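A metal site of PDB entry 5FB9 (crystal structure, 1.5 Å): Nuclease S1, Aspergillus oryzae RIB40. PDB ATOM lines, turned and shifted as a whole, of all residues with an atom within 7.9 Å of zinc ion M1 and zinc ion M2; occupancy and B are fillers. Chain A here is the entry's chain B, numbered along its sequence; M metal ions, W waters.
Zinc ion M1 is bound by a ring nitrogen (ND1) of His 60, water W2, the side-chain carboxylate (OD2) of Asp 119 and a ring nitrogen (NE2) of His 115. Slightly farther from zinc ion M1 lies the side-chain carboxylate (OD1) of Asp 45 (2.7 Å).
The nearest printed residue that does not touch zinc ion M1 is His 125 (4.2 Å).
Zinc ion M2 is bound by NE2 of His 6, water W2, OD1 of Asp 119, N of Trp 1 and O of Trp 1.
The side-chain amino group of Lys 48 lies within salt-bridge range of the side-chain carboxylate of Asp 45, at 2.9 Å. A ring nitrogen (ND1) of His 60 sits close to the side-chain carboxylate (OD1) of Asp 45 (3.1 Å). ND1 of His 6 sits at hydrogen-bond distance from ND1 of His 115 (3.3 Å). ND1 of His 115 lies within hydrogen-bond range of O of Ala 41 (2.7 Å). A ring nitrogen (NE2) of His 115 sits close to the side-chain carboxylate (OD1) of Asp 45 (3.2 Å). N of Trp 1 sits close to OD1 of Asp 152 (3.0 Å). NE1 of Trp 1 sits at hydrogen-bond distance from O of Gly 118 (2.8 Å). A ring nitrogen (ND1) of His 125 lies within hydrogen-bond range of the backbone carbonyl oxygen (O) of His 60 (2.7 Å).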
ATOM      1  N   TRP A   1      -5.124  17.386  13.705  1.00  0.00           N
ATOM      2  CA  TRP A   1      -5.765  16.022  13.785  1.00  0.00           C
ATOM      3  C   TRP A   1      -6.568  15.915  15.051  1.00  0.00           C
ATOM      4  O   TRP A   1      -6.367  16.650  16.005  1.00  0.00           O
ATOM      5  CB  TRP A   1      -4.712  14.872  13.805  1.00  0.00           C
ATOM      6  CG  TRP A   1      -3.679  14.951  12.778  1.00  0.00           C
ATOM      7  CD1 TRP A   1      -2.421  15.454  12.946  1.00  0.00           C
ATOM      8  CD2 TRP A   1      -3.753  14.557  11.435  1.00  0.00           C
ATOM      9  NE1 TRP A   1      -1.713  15.418  11.818  1.00  0.00           N
ATOM     10  CE2 TRP A   1      -2.495  14.843  10.843  1.00  0.00           C
ATOM     11  CE3 TRP A   1      -4.745  13.994  10.642  1.00  0.00           C
ATOM     12  CZ2 TRP A   1      -2.242  14.614   9.491  1.00  0.00           C
ATOM     13  CZ3 TRP A   1      -4.492  13.765   9.314  1.00  0.00           C
ATOM     14  CH2 TRP A   1      -3.256  14.071   8.739  1.00  0.00           C
ATOM     15  N   GLY A   2      -7.442  14.929  15.069  1.00  0.00           N
ATOM     16  CA  GLY A   2      -8.089  14.499  16.301  1.00  0.00           C
ATOM     17  C   GLY A   2      -7.165  13.652  17.139  1.00  0.00           C
ATOM     18  O   GLY A   2      -5.971  13.472  16.796  1.00  0.00           O
ATOM     19  N   ASN A   3      -7.699  13.052  18.201  1.00  0.00           N
ATOM     20  CA  ASN A   3      -6.841  12.360  19.170  1.00  0.00           C
ATOM     21  C   ASN A   3      -6.094  11.217  18.534  1.00  0.00           C
ATOM     22  O   ASN A   3      -4.915  10.996  18.838  1.00  0.00           O
ATOM     23  CB  ASN A   3      -7.673  11.862  20.347  1.00  0.00           C
ATOM     24  CG  ASN A   3      -8.162  12.968  21.245  1.00  0.00           C
ATOM     25  OD1 ASN A   3      -7.892  14.159  21.068  1.00  0.00           O
ATOM     26  ND2 ASN A   3      -8.919  12.551  22.245  1.00  0.00           N
ATOM     27  N   GLY A   5      -5.061  10.722  15.498  1.00  0.00           N
ATOM     28  CA  GLY A   5      -3.931  11.182  14.676  1.00  0.00           C
ATOM     29  C   GLY A   5      -2.760  11.588  15.537  1.00  0.00           C
ATOM     30  O   GLY A   5      -1.626  11.193  15.274  1.00  0.00           O
ATOM     31  N   HIS A   6      -3.006  12.371  16.581  1.00  0.00           N
ATOM     32  CA  HIS A   6      -1.955  12.793  17.460  1.00  0.00           C
ATOM     33  C   HIS A   6      -1.261  11.673  18.200  1.00  0.00           C
ATOM     34  O   HIS A   6      -0.017  11.674  18.354  1.00  0.00           O
ATOM     35  CB  HIS A   6      -2.456  13.846  18.450  1.00  0.00           C
ATOM     36  CG  HIS A   6      -2.662  15.165  17.799  1.00  0.00           C
ATOM     37  ND1 HIS A   6      -1.595  15.957  17.407  1.00  0.00           N
ATOM     38  CD2 HIS A   6      -3.772  15.776  17.325  1.00  0.00           C
ATOM     39  CE1 HIS A   6      -2.034  17.007  16.742  1.00  0.00           C
ATOM     40  NE2 HIS A   6      -3.354  16.953  16.720  1.00  0.00           N
ATOM     41  N   ALA A  41      -0.109  13.475  23.922  1.00  0.00           N
ATOM     42  CA  ALA A  41      -0.200  14.047  22.546  1.00  0.00           C
ATOM     43  C   ALA A  41      -1.483  14.822  22.262  1.00  0.00           C
ATOM     44  O   ALA A  41      -1.543  15.596  21.298  1.00  0.00           O
ATOM     45  CB  ALA A  41      -0.019  12.911  21.532  1.00  0.00           C
ATOM     46  N   THR A  42      -2.533  14.615  23.071  1.00  0.00           N
ATOM     47  CA  THR A  42      -3.826  15.289  22.912  1.00  0.00           C
ATOM     48  C   THR A  42      -4.008  16.425  23.901  1.00  0.00           C
ATOM     49  O   THR A  42      -5.014  17.138  23.805  1.00  0.00           O
ATOM     50  CB  THR A  42      -5.029  14.332  23.129  1.00  0.00           C
ATOM     51  OG1 THR A  42      -5.187  14.018  24.519  1.00  0.00           O
ATOM     52  CG2 THR A  42      -4.853  13.071  22.317  1.00  0.00           C
ATOM     53  N   ALA A  44      -2.902  19.430  24.278  1.00  0.00           N
ATOM     54  CA  ALA A  44      -3.106  20.759  23.769  1.00  0.00           C
ATOM     55  C   ALA A  44      -4.540  20.965  23.301  1.00  0.00           C
ATOM     56  O   ALA A  44      -5.073  22.064  23.389  1.00  0.00           O
ATOM     57  CB  ALA A  44      -2.110  21.104  22.661  1.00  0.00           C
ATOM     58  N   ASP A  45      -5.170  19.899  22.839  1.00  0.00           N
ATOM     59  CA  ASP A  45      -6.549  19.992  22.339  1.00  0.00           C
ATOM     60  C   ASP A  45      -7.578  20.065  23.469  1.00  0.00           C
ATOM     61  O   ASP A  45      -8.709  20.424  23.181  1.00  0.00           O
ATOM     62  CB  ASP A  45      -6.865  18.862  21.356  1.00  0.00           C
ATOM     63  CG  ASP A  45      -6.449  19.184  19.933  1.00  0.00           C
ATOM     64  OD1 ASP A  45      -6.051  20.347  19.656  1.00  0.00           O
ATOM     65  OD2 ASP A  45      -6.550  18.272  19.067  1.00  0.00           O
ATOM     66  N   THR A  46      -7.243  19.646  24.675  1.00  0.00           N
ATOM     67  CA  THR A  46      -8.111  19.861  25.852  1.00  0.00           C
ATOM     68  C   THR A  46      -7.822  21.233  26.444  1.00  0.00           C
ATOM     69  O   THR A  46      -8.747  21.985  26.789  1.00  0.00           O
ATOM     70  CB  THR A  46      -7.927  18.790  26.922  1.00  0.00           C
ATOM     71  OG1 THR A  46      -8.063  17.483  26.371  1.00  0.00           O
ATOM     72  CG2 THR A  46      -8.986  18.948  27.974  1.00  0.00           C
ATOM     73  N   LYS A  48      -6.873  24.029  25.229  1.00  0.00           N
ATOM     74  CA  LYS A  48      -7.324  25.180  24.444  1.00  0.00           C
ATOM     75  C   LYS A  48      -8.784  25.587  24.768  1.00  0.00           C
ATOM     76  O   LYS A  48      -9.196  26.667  24.375  1.00  0.00           O
ATOM     77  CB  LYS A  48      -7.157  24.983  22.940  1.00  0.00           C
ATOM     78  CG  LYS A  48      -8.106  23.956  22.329  1.00  0.00           C
ATOM     79  CD  LYS A  48      -7.733  23.647  20.890  1.00  0.00           C
ATOM     80  CE  LYS A  48      -8.639  22.644  20.264  1.00  0.00           C
ATOM     81  NZ  LYS A  48      -8.167  22.231  18.900  1.00  0.00           N
ATOM     82  N   SER A  56      -3.770  29.702  23.382  1.00  0.00           N
ATOM     83  CA  SER A  56      -2.992  28.708  22.607  1.00  0.00           C
ATOM     84  C   SER A  56      -3.770  28.155  21.415  1.00  0.00           C
ATOM     85  O   SER A  56      -3.225  27.373  20.647  1.00  0.00           O
ATOM     86  CB  SER A  56      -2.470  27.606  23.514  1.00  0.00           C
ATOM     87  OG  SER A  56      -3.482  26.691  23.954  1.00  0.00           O
ATOM     88  N   LYS A  57      -5.047  28.494  21.289  1.00  0.00           N
ATOM     89  CA  LYS A  57      -5.822  28.074  20.115  1.00  0.00           C
ATOM     90  C   LYS A  57      -5.165  28.304  18.748  1.00  0.00           C
ATOM     91  O   LYS A  57      -5.117  27.397  17.891  1.00  0.00           O
ATOM     92  CB  LYS A  57      -7.195  28.727  20.103  1.00  0.00           C
ATOM     93  CG  LYS A  57      -8.144  28.222  21.175  1.00  0.00           C
ATOM     94  CD  LYS A  57      -9.341  29.160  21.280  1.00  0.00           C
ATOM     95  CE  LYS A  57     -10.283  28.867  22.462  1.00  0.00           C
ATOM     96  NZ  LYS A  57     -10.938  27.557  22.205  1.00  0.00           N
ATOM     97  N   TYR A  59      -2.126  28.349  17.986  1.00  0.00           N
ATOM     98  CA  TYR A  59      -0.888  27.599  17.900  1.00  0.00           C
ATOM     99  C   TYR A  59      -1.040  26.266  17.147  1.00  0.00           C
ATOM    100  O   TYR A  59      -0.061  25.586  16.912  1.00  0.00           O
ATOM    101  CB  TYR A  59      -0.248  27.349  19.260  1.00  0.00           C
ATOM    102  CG  TYR A  59       0.077  28.610  20.073  1.00  0.00           C
ATOM    103  CD1 TYR A  59       0.019  29.889  19.525  1.00  0.00           C
ATOM    104  CD2 TYR A  59       0.518  28.469  21.354  1.00  0.00           C
ATOM    105  CE1 TYR A  59       0.338  31.006  20.303  1.00  0.00           C
ATOM    106  CE2 TYR A  59       0.837  29.562  22.137  1.00  0.00           C
ATOM    107  CZ  TYR A  59       0.762  30.805  21.595  1.00  0.00           C
ATOM    108  OH  TYR A  59       1.115  31.907  22.425  1.00  0.00           O
ATOM    109  N   HIS A  60      -2.254  25.895  16.761  1.00  0.00           N
ATOM    110  CA  HIS A  60      -2.474  24.649  16.062  1.00  0.00           C
ATOM    111  C   HIS A  60      -2.400  24.821  14.543  1.00  0.00           C
ATOM    112  O   HIS A  60      -2.418  23.823  13.805  1.00  0.00           O
ATOM    113  CB  HIS A  60      -3.858  24.106  16.493  1.00  0.00           C
ATOM    114  CG  HIS A  60      -3.933  23.764  17.945  1.00  0.00           C
ATOM    115  ND1 HIS A  60      -4.121  22.482  18.443  1.00  0.00           N
ATOM    116  CD2 HIS A  60      -3.771  24.546  19.040  1.00  0.00           C
ATOM    117  CE1 HIS A  60      -4.112  22.502  19.754  1.00  0.00           C
ATOM    118  NE2 HIS A  60      -3.850  23.732  20.141  1.00  0.00           N
ATOM    119  N   PHE A  61      -2.293  26.073  14.074  1.00  0.00           N
ATOM    120  CA  PHE A  61      -2.524  26.420  12.668  1.00  0.00           C
ATOM    121  C   PHE A  61      -1.480  27.378  12.164  1.00  0.00           C
ATOM    122  O   PHE A  61      -0.926  28.162  12.934  1.00  0.00           O
ATOM    123  CB  PHE A  61      -3.880  27.189  12.469  1.00  0.00           C
ATOM    124  CG  PHE A  61      -5.069  26.524  13.114  1.00  0.00           C
ATOM    125  CD1 PHE A  61      -5.604  25.363  12.571  1.00  0.00           C
ATOM    126  CD2 PHE A  61      -5.672  27.081  14.219  1.00  0.00           C
ATOM    127  CE1 PHE A  61      -6.717  24.769  13.145  1.00  0.00           C
ATOM    128  CE2 PHE A  61      -6.766  26.471  14.813  1.00  0.00           C
ATOM    129  CZ  PHE A  61      -7.267  25.300  14.282  1.00  0.00           C
ATOM    130  N   HIS A 115       2.375  17.662  20.206  1.00  0.00           N
ATOM    131  CA  HIS A 115       1.107  17.914  19.501  1.00  0.00           C
ATOM    132  C   HIS A 115       1.266  18.705  18.195  1.00  0.00           C
ATOM    133  O   HIS A 115       0.714  18.345  17.161  1.00  0.00           O
ATOM    134  CB  HIS A 115       0.161  18.685  20.439  1.00  0.00           C
ATOM    135  CG  HIS A 115      -1.200  18.897  19.886  1.00  0.00           C
ATOM    136  ND1 HIS A 115      -2.194  17.937  20.016  1.00  0.00           N
ATOM    137  CD2 HIS A 115      -1.725  19.915  19.153  1.00  0.00           C
ATOM    138  CE1 HIS A 115      -3.288  18.396  19.409  1.00  0.00           C
ATOM    139  NE2 HIS A 115      -3.014  19.574  18.876  1.00  0.00           N
ATOM    140  N   ILE A 116       1.962  19.824  18.290  1.00  0.00           N
ATOM    141  CA  ILE A 116       1.978  20.825  17.196  1.00  0.00           C
ATOM    142  C   ILE A 116       2.767  20.289  16.003  1.00  0.00           C
ATOM    143  O   ILE A 116       2.361  20.503  14.862  1.00  0.00           O
ATOM    144  CB  ILE A 116       2.423  22.196  17.649  1.00  0.00           C
ATOM    145  CG1 ILE A 116       1.458  22.705  18.703  1.00  0.00           C
ATOM    146  CG2 ILE A 116       2.590  23.126  16.467  1.00  0.00           C
ATOM    147  CD1 ILE A 116       1.908  24.015  19.361  1.00  0.00           C
ATOM    148  N   GLY A 118       2.619  17.286  15.087  1.00  0.00           N
ATOM    149  CA  GLY A 118       1.508  16.570  14.445  1.00  0.00           C
ATOM    150  C   GLY A 118       0.594  17.509  13.589  1.00  0.00           C
ATOM    151  O   GLY A 118       0.352  17.253  12.403  1.00  0.00           O
ATOM    152  N   ASP A 119       0.135  18.610  14.183  1.00  0.00           N
ATOM    153  CA  ASP A 119      -0.756  19.505  13.465  1.00  0.00           C
ATOM    154  C   ASP A 119      -0.150  20.126  12.220  1.00  0.00           C
ATOM    155  O   ASP A 119      -0.856  20.299  11.232  1.00  0.00           O
ATOM    156  CB  ASP A 119      -1.300  20.627  14.366  1.00  0.00           C
ATOM    157  CG  ASP A 119      -2.521  20.211  15.167  1.00  0.00           C
ATOM    158  OD1 ASP A 119      -3.159  19.224  14.839  1.00  0.00           O
ATOM    159  OD2 ASP A 119      -2.819  20.923  16.149  1.00  0.00           O
ATOM    160  N   ILE A 120       1.141  20.440  12.214  1.00  0.00           N
ATOM    161  CA  ILE A 120       1.786  21.004  11.037  1.00  0.00           C
ATOM    162  C   ILE A 120       1.667  20.081   9.846  1.00  0.00           C
ATOM    163  O   ILE A 120       1.709  20.520   8.695  1.00  0.00           O
ATOM    164  CB  ILE A 120       3.218  21.373  11.397  1.00  0.00           C
ATOM    165  CG1 ILE A 120       3.232  22.612  12.314  1.00  0.00           C
ATOM    166  CG2 ILE A 120       4.028  21.600  10.169  1.00  0.00           C
ATOM    167  CD1 ILE A 120       4.602  22.787  13.027  1.00  0.00           C
ATOM    168  N   GLN A 122      -1.039  18.134   9.162  1.00  0.00           N
ATOM    169  CA  GLN A 122      -2.426  18.043   8.681  1.00  0.00           C
ATOM    170  C   GLN A 122      -2.584  19.194   7.699  1.00  0.00           C
ATOM    171  O   GLN A 122      -2.521  20.367   8.125  1.00  0.00           O
ATOM    172  CB  GLN A 122      -3.388  18.160   9.878  1.00  0.00           C
ATOM    173  CG  GLN A 122      -4.777  17.504   9.750  1.00  0.00           C
ATOM    174  CD  GLN A 122      -5.733  18.162   8.754  1.00  0.00           C
ATOM    175  OE1 GLN A 122      -5.369  18.389   7.625  1.00  0.00           O
ATOM    176  NE2 GLN A 122      -6.947  18.484   9.214  1.00  0.00           N
ATOM    177  N   HIS A 125      -4.586  22.218   8.496  1.00  0.00           N
ATOM    178  CA  HIS A 125      -4.041  23.105   9.570  1.00  0.00           C
ATOM    179  C   HIS A 125      -3.032  24.125   9.030  1.00  0.00           C
ATOM    180  O   HIS A 125      -2.569  24.978   9.798  1.00  0.00           O
ATOM    181  CB  HIS A 125      -3.388  22.272  10.678  1.00  0.00           C
ATOM    182  CG  HIS A 125      -4.383  21.748  11.650  1.00  0.00           C
ATOM    183  ND1 HIS A 125      -4.317  22.036  12.983  1.00  0.00           N
ATOM    184  CD2 HIS A 125      -5.450  20.932  11.495  1.00  0.00           C
ATOM    185  CE1 HIS A 125      -5.363  21.515  13.602  1.00  0.00           C
ATOM    186  NE2 HIS A 125      -6.059  20.840  12.727  1.00  0.00           N
ATOM    187  N   HIS A 148     -12.537  20.118   6.930  1.00  0.00           N
ATOM    188  CA  HIS A 148     -11.504  20.056   7.933  1.00  0.00           C
ATOM    189  C   HIS A 148     -11.672  18.811   8.826  1.00  0.00           C
ATOM    190  O   HIS A 148     -10.698  18.069   9.063  1.00  0.00           O
ATOM    191  CB  HIS A 148     -11.528  21.323   8.803  1.00  0.00           C
ATOM    192  CG  HIS A 148     -10.368  21.408   9.707  1.00  0.00           C
ATOM    193  ND1 HIS A 148      -9.261  22.188   9.465  1.00  0.00           N
ATOM    194  CD2 HIS A 148     -10.137  20.765  10.860  1.00  0.00           C
ATOM    195  CE1 HIS A 148      -8.389  22.028  10.453  1.00  0.00           C
ATOM    196  NE2 HIS A 148      -8.893  21.155  11.314  1.00  0.00           N
ATOM    197  N   ASP A 152      -9.237  15.656   9.945  1.00  0.00           N
ATOM    198  CA  ASP A 152      -8.775  15.525  11.315  1.00  0.00           C
ATOM    199  C   ASP A 152      -9.123  14.115  11.868  1.00  0.00           C
ATOM    200  O   ASP A 152      -8.348  13.550  12.631  1.00  0.00           O
ATOM    201  CB  ASP A 152      -9.429  16.542  12.244  1.00  0.00           C
ATOM    202  CG  ASP A 152      -8.680  17.839  12.373  1.00  0.00           C
ATOM    203  OD1 ASP A 152      -7.510  17.994  11.984  1.00  0.00           O
ATOM    204  OD2 ASP A 152      -9.320  18.727  12.964  1.00  0.00           O
ATOM    205  N   THR A 153     -10.289  13.604  11.483  1.00  0.00           N
ATOM    206  CA  THR A 153     -11.006  12.615  12.266  1.00  0.00           C
ATOM    207  C   THR A 153     -11.638  11.520  11.424  1.00  0.00           C
ATOM    208  O   THR A 153     -11.245  10.365  11.549  1.00  0.00           O
ATOM    209  CB  THR A 153     -12.046  13.326  13.144  1.00  0.00           C
ATOM    210  OG1 THR A 153     -11.334  14.114  14.135  1.00  0.00           O
ATOM    211  CG2 THR A 153     -12.923  12.376  13.890  1.00  0.00           C
HETATM  212 ZN    ZN M   1      -4.245  20.670  17.611  1.00  0.00          ZN
HETATM  213 ZN    ZN M   2      -4.701  18.053  15.668  1.00  0.00          ZN
HETATM  214 ZN    ZN M   3      -8.052  20.338  13.104  1.00  0.00          ZN
HETATM  215  O   HOH W   1      -6.875  22.705  16.574  1.00  0.00           O
HETATM  216  O   HOH W   2      -5.647  19.451  16.849  1.00  0.00           O
HETATM  217  O   HOH W   3      -7.539  19.561  14.884  1.00  0.00           O
